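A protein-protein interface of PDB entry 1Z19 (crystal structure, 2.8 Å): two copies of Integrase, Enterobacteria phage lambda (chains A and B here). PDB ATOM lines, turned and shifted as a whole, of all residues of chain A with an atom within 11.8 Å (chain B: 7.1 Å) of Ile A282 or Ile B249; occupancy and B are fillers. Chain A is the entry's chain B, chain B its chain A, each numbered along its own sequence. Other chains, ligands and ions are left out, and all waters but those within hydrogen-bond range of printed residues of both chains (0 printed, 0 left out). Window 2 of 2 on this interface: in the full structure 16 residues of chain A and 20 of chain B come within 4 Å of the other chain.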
ATOM      1  N   GLU A 246       7.525  23.304 -14.395  1.00  0.00           N
ATOM      2  CA  GLU A 246       6.224  23.527 -15.017  1.00  0.00           C
ATOM      3  C   GLU A 246       5.347  22.304 -14.768  1.00  0.00           C
ATOM      4  O   GLU A 246       4.283  22.398 -14.165  1.00  0.00           O
ATOM      5  CB  GLU A 246       6.415  23.731 -16.527  1.00  0.00           C
ATOM      6  CG  GLU A 246       5.145  23.768 -17.391  1.00  0.00           C
ATOM      7  CD  GLU A 246       4.477  25.129 -17.394  1.00  0.00           C
ATOM      8  OE1 GLU A 246       3.631  25.395 -18.280  1.00  0.00           O
ATOM      9  OE2 GLU A 246       4.800  25.937 -16.501  1.00  0.00           O
ATOM     10  N   LYS A 247       5.819  21.150 -15.222  1.00  0.00           N
ATOM     11  CA  LYS A 247       5.082  19.902 -15.080  1.00  0.00           C
ATOM     12  C   LYS A 247       4.999  19.346 -13.667  1.00  0.00           C
ATOM     13  O   LYS A 247       4.068  18.609 -13.356  1.00  0.00           O
ATOM     14  CB  LYS A 247       5.688  18.836 -15.996  1.00  0.00           C
ATOM     15  CG  LYS A 247       5.555  19.123 -17.483  1.00  0.00           C
ATOM     16  CD  LYS A 247       6.014  17.920 -18.299  1.00  0.00           C
ATOM     17  CE  LYS A 247       5.796  18.129 -19.798  1.00  0.00           C
ATOM     18  NZ  LYS A 247       5.975  16.856 -20.573  1.00  0.00           N
ATOM     19  N   ILE A 249       5.254  21.325 -10.548  1.00  0.00           N
ATOM     20  CA  ILE A 249       4.512  22.186  -9.650  1.00  0.00           C
ATOM     21  C   ILE A 249       3.452  22.980 -10.394  1.00  0.00           C
ATOM     22  O   ILE A 249       2.270  22.650 -10.328  1.00  0.00           O
ATOM     23  CB  ILE A 249       5.456  23.134  -8.943  1.00  0.00           C
ATOM     24  CG1 ILE A 249       6.449  22.316  -8.111  1.00  0.00           C
ATOM     25  CG2 ILE A 249       4.664  24.126  -8.116  1.00  0.00           C
ATOM     26  CD1 ILE A 249       7.389  23.144  -7.281  1.00  0.00           C
ATOM     27  N   ASP A 278       5.312  16.646 -25.994  1.00  0.00           N
ATOM     28  CA  ASP A 278       4.707  17.068 -24.744  1.00  0.00           C
ATOM     29  C   ASP A 278       3.548  16.161 -24.356  1.00  0.00           C
ATOM     30  O   ASP A 278       2.464  16.270 -24.918  1.00  0.00           O
ATOM     31  CB  ASP A 278       4.238  18.513 -24.891  1.00  0.00           C
ATOM     32  CG  ASP A 278       3.835  19.125 -23.581  1.00  0.00           C
ATOM     33  OD1 ASP A 278       4.570  18.914 -22.588  1.00  0.00           O
ATOM     34  OD2 ASP A 278       2.795  19.825 -23.544  1.00  0.00           O
ATOM     35  N   LYS A 279       3.784  15.264 -23.401  1.00  0.00           N
ATOM     36  CA  LYS A 279       2.744  14.342 -22.952  1.00  0.00           C
ATOM     37  C   LYS A 279       1.726  15.093 -22.105  1.00  0.00           C
ATOM     38  O   LYS A 279       1.989  15.413 -20.954  1.00  0.00           O
ATOM     39  CB  LYS A 279       3.349  13.184 -22.143  1.00  0.00           C
ATOM     40  CG  LYS A 279       4.407  12.366 -22.914  1.00  0.00           C
ATOM     41  CD  LYS A 279       4.507  10.923 -22.417  1.00  0.00           C
ATOM     42  CE  LYS A 279       3.258  10.120 -22.772  1.00  0.00           C
ATOM     43  NZ  LYS A 279       3.216   8.794 -22.090  1.00  0.00           N
ATOM     44  N   ILE A 280       0.565  15.368 -22.691  1.00  0.00           N
ATOM     45  CA  ILE A 280      -0.494  16.116 -22.025  1.00  0.00           C
ATOM     46  C   ILE A 280      -1.167  15.416 -20.854  1.00  0.00           C
ATOM     47  O   ILE A 280      -1.738  14.325 -20.998  1.00  0.00           O
ATOM     48  CB  ILE A 280      -1.581  16.532 -23.034  1.00  0.00           C
ATOM     49  CG1 ILE A 280      -0.988  17.526 -24.034  1.00  0.00           C
ATOM     50  CG2 ILE A 280      -2.783  17.115 -22.299  1.00  0.00           C
ATOM     51  CD1 ILE A 280      -1.909  17.876 -25.172  1.00  0.00           C
ATOM     52  N   GLU A 281      -1.108  16.077 -19.699  1.00  0.00           N
ATOM     53  CA  GLU A 281      -1.692  15.578 -18.451  1.00  0.00           C
ATOM     54  C   GLU A 281      -3.082  16.164 -18.234  1.00  0.00           C
ATOM     55  O   GLU A 281      -3.358  17.305 -18.608  1.00  0.00           O
ATOM     56  CB  GLU A 281      -0.793  15.952 -17.263  1.00  0.00           C
ATOM     57  CG  GLU A 281       0.510  15.163 -17.151  1.00  0.00           C
ATOM     58  CD  GLU A 281       1.573  15.884 -16.314  1.00  0.00           C
ATOM     59  OE1 GLU A 281       1.235  16.425 -15.231  1.00  0.00           O
ATOM     60  OE2 GLU A 281       2.753  15.902 -16.740  1.00  0.00           O
ATOM     61  N   ILE A 282      -3.951  15.376 -17.623  1.00  0.00           N
ATOM     62  CA  ILE A 282      -5.302  15.835 -17.353  1.00  0.00           C
ATOM     63  C   ILE A 282      -5.289  16.487 -15.980  1.00  0.00           C
ATOM     64  O   ILE A 282      -5.835  15.954 -15.023  1.00  0.00           O
ATOM     65  CB  ILE A 282      -6.273  14.656 -17.358  1.00  0.00           C
ATOM     66  CG1 ILE A 282      -6.044  13.838 -18.638  1.00  0.00           C
ATOM     67  CG2 ILE A 282      -7.703  15.164 -17.303  1.00  0.00           C
ATOM     68  CD1 ILE A 282      -6.897  12.607 -18.742  1.00  0.00           C
ATOM     69  N   LYS A 283      -4.654  17.646 -15.890  1.00  0.00           N
ATOM     70  CA  LYS A 283      -4.556  18.364 -14.625  1.00  0.00           C
ATOM     71  C   LYS A 283      -5.300  19.702 -14.712  1.00  0.00           C
ATOM     72  O   LYS A 283      -4.714  20.759 -14.386  1.00  0.00           O
ATOM     73  CB  LYS A 283      -3.073  18.587 -14.276  1.00  0.00           C
ATOM     74  CG  LYS A 283      -2.805  19.091 -12.858  1.00  0.00           C
ATOM     75  CD  LYS A 283      -1.314  19.367 -12.615  1.00  0.00           C
ATOM     76  CE  LYS A 283      -0.441  18.120 -12.835  1.00  0.00           C
ATOM     77  NZ  LYS A 283       1.009  18.362 -12.525  1.00  0.00           N
ATOM     78  OXT LYS A 283      -6.479  19.674 -15.106  1.00  0.00           O
ATOM     79  N   PRO B 170      -3.551  11.780 -24.573  1.00  0.00           N
ATOM     80  CA  PRO B 170      -3.955  10.527 -23.927  1.00  0.00           C
ATOM     81  C   PRO B 170      -5.310  10.062 -24.454  1.00  0.00           C
ATOM     82  O   PRO B 170      -6.297  10.792 -24.397  1.00  0.00           O
ATOM     83  CB  PRO B 170      -3.984  10.895 -22.448  1.00  0.00           C
ATOM     84  CG  PRO B 170      -4.411  12.315 -22.468  1.00  0.00           C
ATOM     85  CD  PRO B 170      -3.633  12.911 -23.627  1.00  0.00           C
ATOM     86  N   ALA B 172      -7.699   8.730 -23.464  1.00  0.00           N
ATOM     87  CA  ALA B 172      -8.670   8.434 -22.434  1.00  0.00           C
ATOM     88  C   ALA B 172      -9.568   9.635 -22.213  1.00  0.00           C
ATOM     89  O   ALA B 172     -10.501   9.576 -21.422  1.00  0.00           O
ATOM     90  CB  ALA B 172      -7.960   8.058 -21.138  1.00  0.00           C
ATOM     91  N   LEU B 173      -9.282  10.729 -22.907  1.00  0.00           N
ATOM     92  CA  LEU B 173     -10.090  11.932 -22.759  1.00  0.00           C
ATOM     93  C   LEU B 173     -11.560  11.624 -22.999  1.00  0.00           C
ATOM     94  O   LEU B 173     -11.896  10.610 -23.606  1.00  0.00           O
ATOM     95  CB  LEU B 173      -9.641  13.012 -23.747  1.00  0.00           C
ATOM     96  CG  LEU B 173      -8.580  14.019 -23.311  1.00  0.00           C
ATOM     97  CD1 LEU B 173      -7.292  13.307 -23.015  1.00  0.00           C
ATOM     98  CD2 LEU B 173      -8.378  15.043 -24.415  1.00  0.00           C
ATOM     99  N   HIS B 174     -12.431  12.505 -22.522  1.00  0.00           N
ATOM    100  CA  HIS B 174     -13.860  12.336 -22.708  1.00  0.00           C
ATOM    101  C   HIS B 174     -14.600  13.660 -22.513  1.00  0.00           C
ATOM    102  O   HIS B 174     -14.463  14.321 -21.485  1.00  0.00           O
ATOM    103  CB  HIS B 174     -14.390  11.254 -21.751  1.00  0.00           C
ATOM    104  CG  HIS B 174     -14.115  11.533 -20.304  1.00  0.00           C
ATOM    105  ND1 HIS B 174     -15.051  12.101 -19.463  1.00  0.00           N
ATOM    106  CD2 HIS B 174     -12.998  11.354 -19.557  1.00  0.00           C
ATOM    107  CE1 HIS B 174     -14.523  12.260 -18.261  1.00  0.00           C
ATOM    108  NE2 HIS B 174     -13.278  11.815 -18.291  1.00  0.00           N
ATOM    109  N   ASP B 176     -17.707  15.423 -21.624  1.00  0.00           N
ATOM    110  CA  ASP B 176     -18.941  15.105 -20.912  1.00  0.00           C
ATOM    111  C   ASP B 176     -20.207  15.664 -21.565  1.00  0.00           C
ATOM    112  O   ASP B 176     -21.137  14.920 -21.879  1.00  0.00           O
ATOM    113  CB  ASP B 176     -18.859  15.590 -19.454  1.00  0.00           C
ATOM    114  CG  ASP B 176     -17.764  14.889 -18.664  1.00  0.00           C
ATOM    115  OD1 ASP B 176     -17.468  13.712 -18.970  1.00  0.00           O
ATOM    116  OD2 ASP B 176     -17.210  15.504 -17.726  1.00  0.00           O
ATOM    117  N   LEU B 244     -15.284  23.629 -23.896  1.00  0.00           N
ATOM    118  CA  LEU B 244     -15.822  22.539 -23.104  1.00  0.00           C
ATOM    119  C   LEU B 244     -14.793  22.043 -22.113  1.00  0.00           C
ATOM    120  O   LEU B 244     -15.069  21.963 -20.912  1.00  0.00           O
ATOM    121  CB  LEU B 244     -16.273  21.385 -24.003  1.00  0.00           C
ATOM    122  CG  LEU B 244     -17.524  21.649 -24.846  1.00  0.00           C
ATOM    123  CD1 LEU B 244     -17.808  20.432 -25.711  1.00  0.00           C
ATOM    124  CD2 LEU B 244     -18.716  21.978 -23.932  1.00  0.00           C
ATOM    125  N   TYR B 245     -13.606  21.710 -22.610  1.00  0.00           N
ATOM    126  CA  TYR B 245     -12.555  21.216 -21.734  1.00  0.00           C
ATOM    127  C   TYR B 245     -12.213  22.273 -20.708  1.00  0.00           C
ATOM    128  O   TYR B 245     -11.842  21.956 -19.586  1.00  0.00           O
ATOM    129  CB  TYR B 245     -11.298  20.839 -22.531  1.00  0.00           C
ATOM    130  CG  TYR B 245     -11.332  19.454 -23.145  1.00  0.00           C
ATOM    131  CD1 TYR B 245     -11.635  18.336 -22.374  1.00  0.00           C
ATOM    132  CD2 TYR B 245     -11.062  19.264 -24.500  1.00  0.00           C
ATOM    133  CE1 TYR B 245     -11.668  17.058 -22.934  1.00  0.00           C
ATOM    134  CE2 TYR B 245     -11.089  17.985 -25.074  1.00  0.00           C
ATOM    135  CZ  TYR B 245     -11.395  16.889 -24.287  1.00  0.00           C
ATOM    136  OH  TYR B 245     -11.427  15.632 -24.847  1.00  0.00           O
ATOM    137  N   GLU B 246     -12.340  23.537 -21.088  1.00  0.00           N
ATOM    138  CA  GLU B 246     -12.028  24.610 -20.164  1.00  0.00           C
ATOM    139  C   GLU B 246     -12.767  24.372 -18.853  1.00  0.00           C
ATOM    140  O   GLU B 246     -12.164  24.369 -17.784  1.00  0.00           O
ATOM    141  CB  GLU B 246     -12.440  25.953 -20.751  1.00  0.00           C
ATOM    142  CG  GLU B 246     -11.824  27.138 -20.041  1.00  0.00           C
ATOM    143  CD  GLU B 246     -12.345  28.471 -20.563  1.00  0.00           C
ATOM    144  OE1 GLU B 246     -12.556  28.584 -21.793  1.00  0.00           O
ATOM    145  OE2 GLU B 246     -12.530  29.408 -19.748  1.00  0.00           O
ATOM    146  N   LYS B 247     -14.075  24.154 -18.939  1.00  0.00           N
ATOM    147  CA  LYS B 247     -14.870  23.923 -17.744  1.00  0.00           C
ATOM    148  C   LYS B 247     -14.679  22.538 -17.143  1.00  0.00           C
ATOM    149  O   LYS B 247     -14.327  22.411 -15.974  1.00  0.00           O
ATOM    150  CB  LYS B 247     -16.353  24.160 -18.029  1.00  0.00           C
ATOM    151  CG  LYS B 247     -16.675  25.605 -18.362  1.00  0.00           C
ATOM    152  CD  LYS B 247     -18.167  25.879 -18.303  1.00  0.00           C
ATOM    153  CE  LYS B 247     -18.464  27.343 -18.604  1.00  0.00           C
ATOM    154  NZ  LYS B 247     -18.062  27.719 -19.996  1.00  0.00           N
ATOM    155  N   GLN B 248     -14.904  21.500 -17.938  1.00  0.00           N
ATOM    156  CA  GLN B 248     -14.760  20.136 -17.447  1.00  0.00           C
ATOM    157  C   GLN B 248     -13.474  19.895 -16.646  1.00  0.00           C
ATOM    158  O   GLN B 248     -13.529  19.541 -15.468  1.00  0.00           O
ATOM    159  CB  GLN B 248     -14.822  19.150 -18.606  1.00  0.00           C
ATOM    160  CG  GLN B 248     -14.775  17.717 -18.149  1.00  0.00           C
ATOM    161  CD  GLN B 248     -14.879  16.732 -19.286  1.00  0.00           C
ATOM    162  OE1 GLN B 248     -15.791  16.814 -20.119  1.00  0.00           O
ATOM    163  NE2 GLN B 248     -13.951  15.779 -19.325  1.00  0.00           N
ATOM    164  N   ILE B 249     -12.324  20.077 -17.288  1.00  0.00           N
ATOM    165  CA  ILE B 249     -11.038  19.875 -16.634  1.00  0.00           C
ATOM    166  C   ILE B 249     -10.466  21.206 -16.182  1.00  0.00           C
ATOM    167  O   ILE B 249     -10.666  21.609 -15.038  1.00  0.00           O
ATOM    168  CB  ILE B 249     -10.046  19.195 -17.570  1.00  0.00           C
ATOM    169  CG1 ILE B 249     -10.632  17.876 -18.053  1.00  0.00           C
ATOM    170  CG2 ILE B 249      -8.752  18.922 -16.846  1.00  0.00           C
ATOM    171  CD1 ILE B 249      -9.793  17.196 -19.101  1.00  0.00           C
ATOM    172  N   SER B 250      -9.752  21.897 -17.060  1.00  0.00           N
ATOM    173  CA  SER B 250      -9.205  23.189 -16.665  1.00  0.00           C
ATOM    174  C   SER B 250      -8.796  24.042 -17.848  1.00  0.00           C
ATOM    175  O   SER B 250      -8.572  23.535 -18.945  1.00  0.00           O
ATOM    176  CB  SER B 250      -8.011  22.997 -15.738  1.00  0.00           C
ATOM    177  OG  SER B 250      -7.000  22.233 -16.362  1.00  0.00           O
ATOM    178  N   ASP B 251      -8.711  25.345 -17.611  1.00  0.00           N
ATOM    179  CA  ASP B 251      -8.329  26.296 -18.644  1.00  0.00           C
ATOM    180  C   ASP B 251      -6.920  25.942 -19.071  1.00  0.00           C
ATOM    181  O   ASP B 251      -6.586  25.987 -20.248  1.00  0.00           O
ATOM    182  CB  ASP B 251      -8.337  27.717 -18.085  1.00  0.00           C
ATOM    183  CG  ASP B 251      -9.449  27.941 -17.060  1.00  0.00           C
ATOM    184  OD1 ASP B 251     -10.641  27.989 -17.453  1.00  0.00           O
ATOM    185  OD2 ASP B 251      -9.123  28.067 -15.854  1.00  0.00           O
ATOM    186  N   LYS B 252      -6.093  25.583 -18.098  1.00  0.00           N
ATOM    187  CA  LYS B 252      -4.715  25.222 -18.387  1.00  0.00           C
ATOM    188  C   LYS B 252      -4.697  24.069 -19.370  1.00  0.00           C
ATOM    189  O   LYS B 252      -3.934  24.069 -20.333  1.00  0.00           O
ATOM    190  CB  LYS B 252      -3.985  24.828 -17.100  1.00  0.00           C
ATOM    191  N   PHE B 253      -5.546  23.084 -19.120  1.00  0.00           N
ATOM    192  CA  PHE B 253      -5.619  21.917 -19.977  1.00  0.00           C
ATOM    193  C   PHE B 253      -6.073  22.271 -21.388  1.00  0.00           C
ATOM    194  O   PHE B 253      -5.487  21.827 -22.363  1.00  0.00           O
ATOM    195  CB  PHE B 253      -6.545  20.888 -19.345  1.00  0.00           C
ATOM    196  CG  PHE B 253      -6.855  19.740 -20.228  1.00  0.00           C
ATOM    197  CD1 PHE B 253      -7.901  19.811 -21.130  1.00  0.00           C
ATOM    198  CD2 PHE B 253      -6.105  18.578 -20.157  1.00  0.00           C
ATOM    199  CE1 PHE B 253      -8.201  18.736 -21.952  1.00  0.00           C
ATOM    200  CE2 PHE B 253      -6.391  17.495 -20.972  1.00  0.00           C
ATOM    201  CZ  PHE B 253      -7.445  17.572 -21.875  1.00  0.00           C
ATOM    202  N   ALA B 254      -7.115  23.076 -21.503  1.00  0.00           N
ATOM    203  CA  ALA B 254      -7.585  23.462 -22.819  1.00  0.00           C
ATOM    204  C   ALA B 254      -6.417  24.005 -23.649  1.00  0.00           C
ATOM    205  O   ALA B 254      -6.299  23.723 -24.838  1.00  0.00           O
ATOM    206  CB  ALA B 254      -8.668  24.509 -22.697  1.00  0.00           C
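The side-chain hydroxyl (OG) of Ser B250 is in hydrogen-bond range of the chain-end carboxylate (OXT) of Lys A283 (2.9 Å).
N of Ser B250 sits at hydrogen-bond distance from O of Tyr B245.
The side-chain amino group (NZ) of Lys A283 is in salt-bridge range of the side-chain carboxylate (OE1) of Glu A281.
O of Lys A247 sits at hydrogen-bond distance from NZ of Lys A283 (3.2 Å).
The side-chain hydroxyl (OG) of Ser B250 sits at hydrogen-bond distance from the backbone NH (N) of Phe B253, at 3.2 Å.
Among the printed residues, merely in contact across the chains: Ile A280 with Pro B170 (3.5 Å), Ile A280 with Phe B253 (3.9 Å), Glu A281 with Phe B253 (3.4 Å), Ile A282 with Ile B249 (3.4 Å) and Lys A283 with Ile B249 (3.0 Å).
Of the printed residues of chain B, Ile A280 touches Pro B170 (3.5 Å) and Phe B253 (3.9 Å).
Of the printed residues of chain B, Ile A282 touches Ile B249.
Printed residues of chain B within 4 Å of Lys A283: Ile B249 and Ser B250.
Of chain A, only Ile A280 comes within 4 Å of Pro B170.
No residue of chain A comes within 4 Å of Ala B172.
No residue of chain A comes within 4 Å of Leu B173.
Of chain A, only Ile A282 (3.4 Å) and Lys A283 (3.0 Å) come within 4 Å of Ile B249.
Of chain A, only Lys A283 comes within 4 Å of Ser B250.
Of the printed residues of chain A, Phe B253 touches Ile A280 (3.9 Å) and Glu A281 (3.4 Å).
The nearest residue of chain A that does not touch Ile B249 is Glu A281 (5.9 Å).
Of the 16 printed residues of chain B, 4 touch a printed residue of chain A.
Printed residues of chain A that touch a printed residue of chain B: Ile A280, Glu A281, Ile A282 and Lys A283.
Hydrophobic or aromatic side chains of chain A that line the printed part of chain B: Ile A280 and Ile A282.
Among the printed residues, 6 pairs touch across the chains.
Positions printed for both chains: 246, 247 and 249.
Of the 6 pairs that touch across the chains among the printed residues, none has its exchanged pair printed and touching as well.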
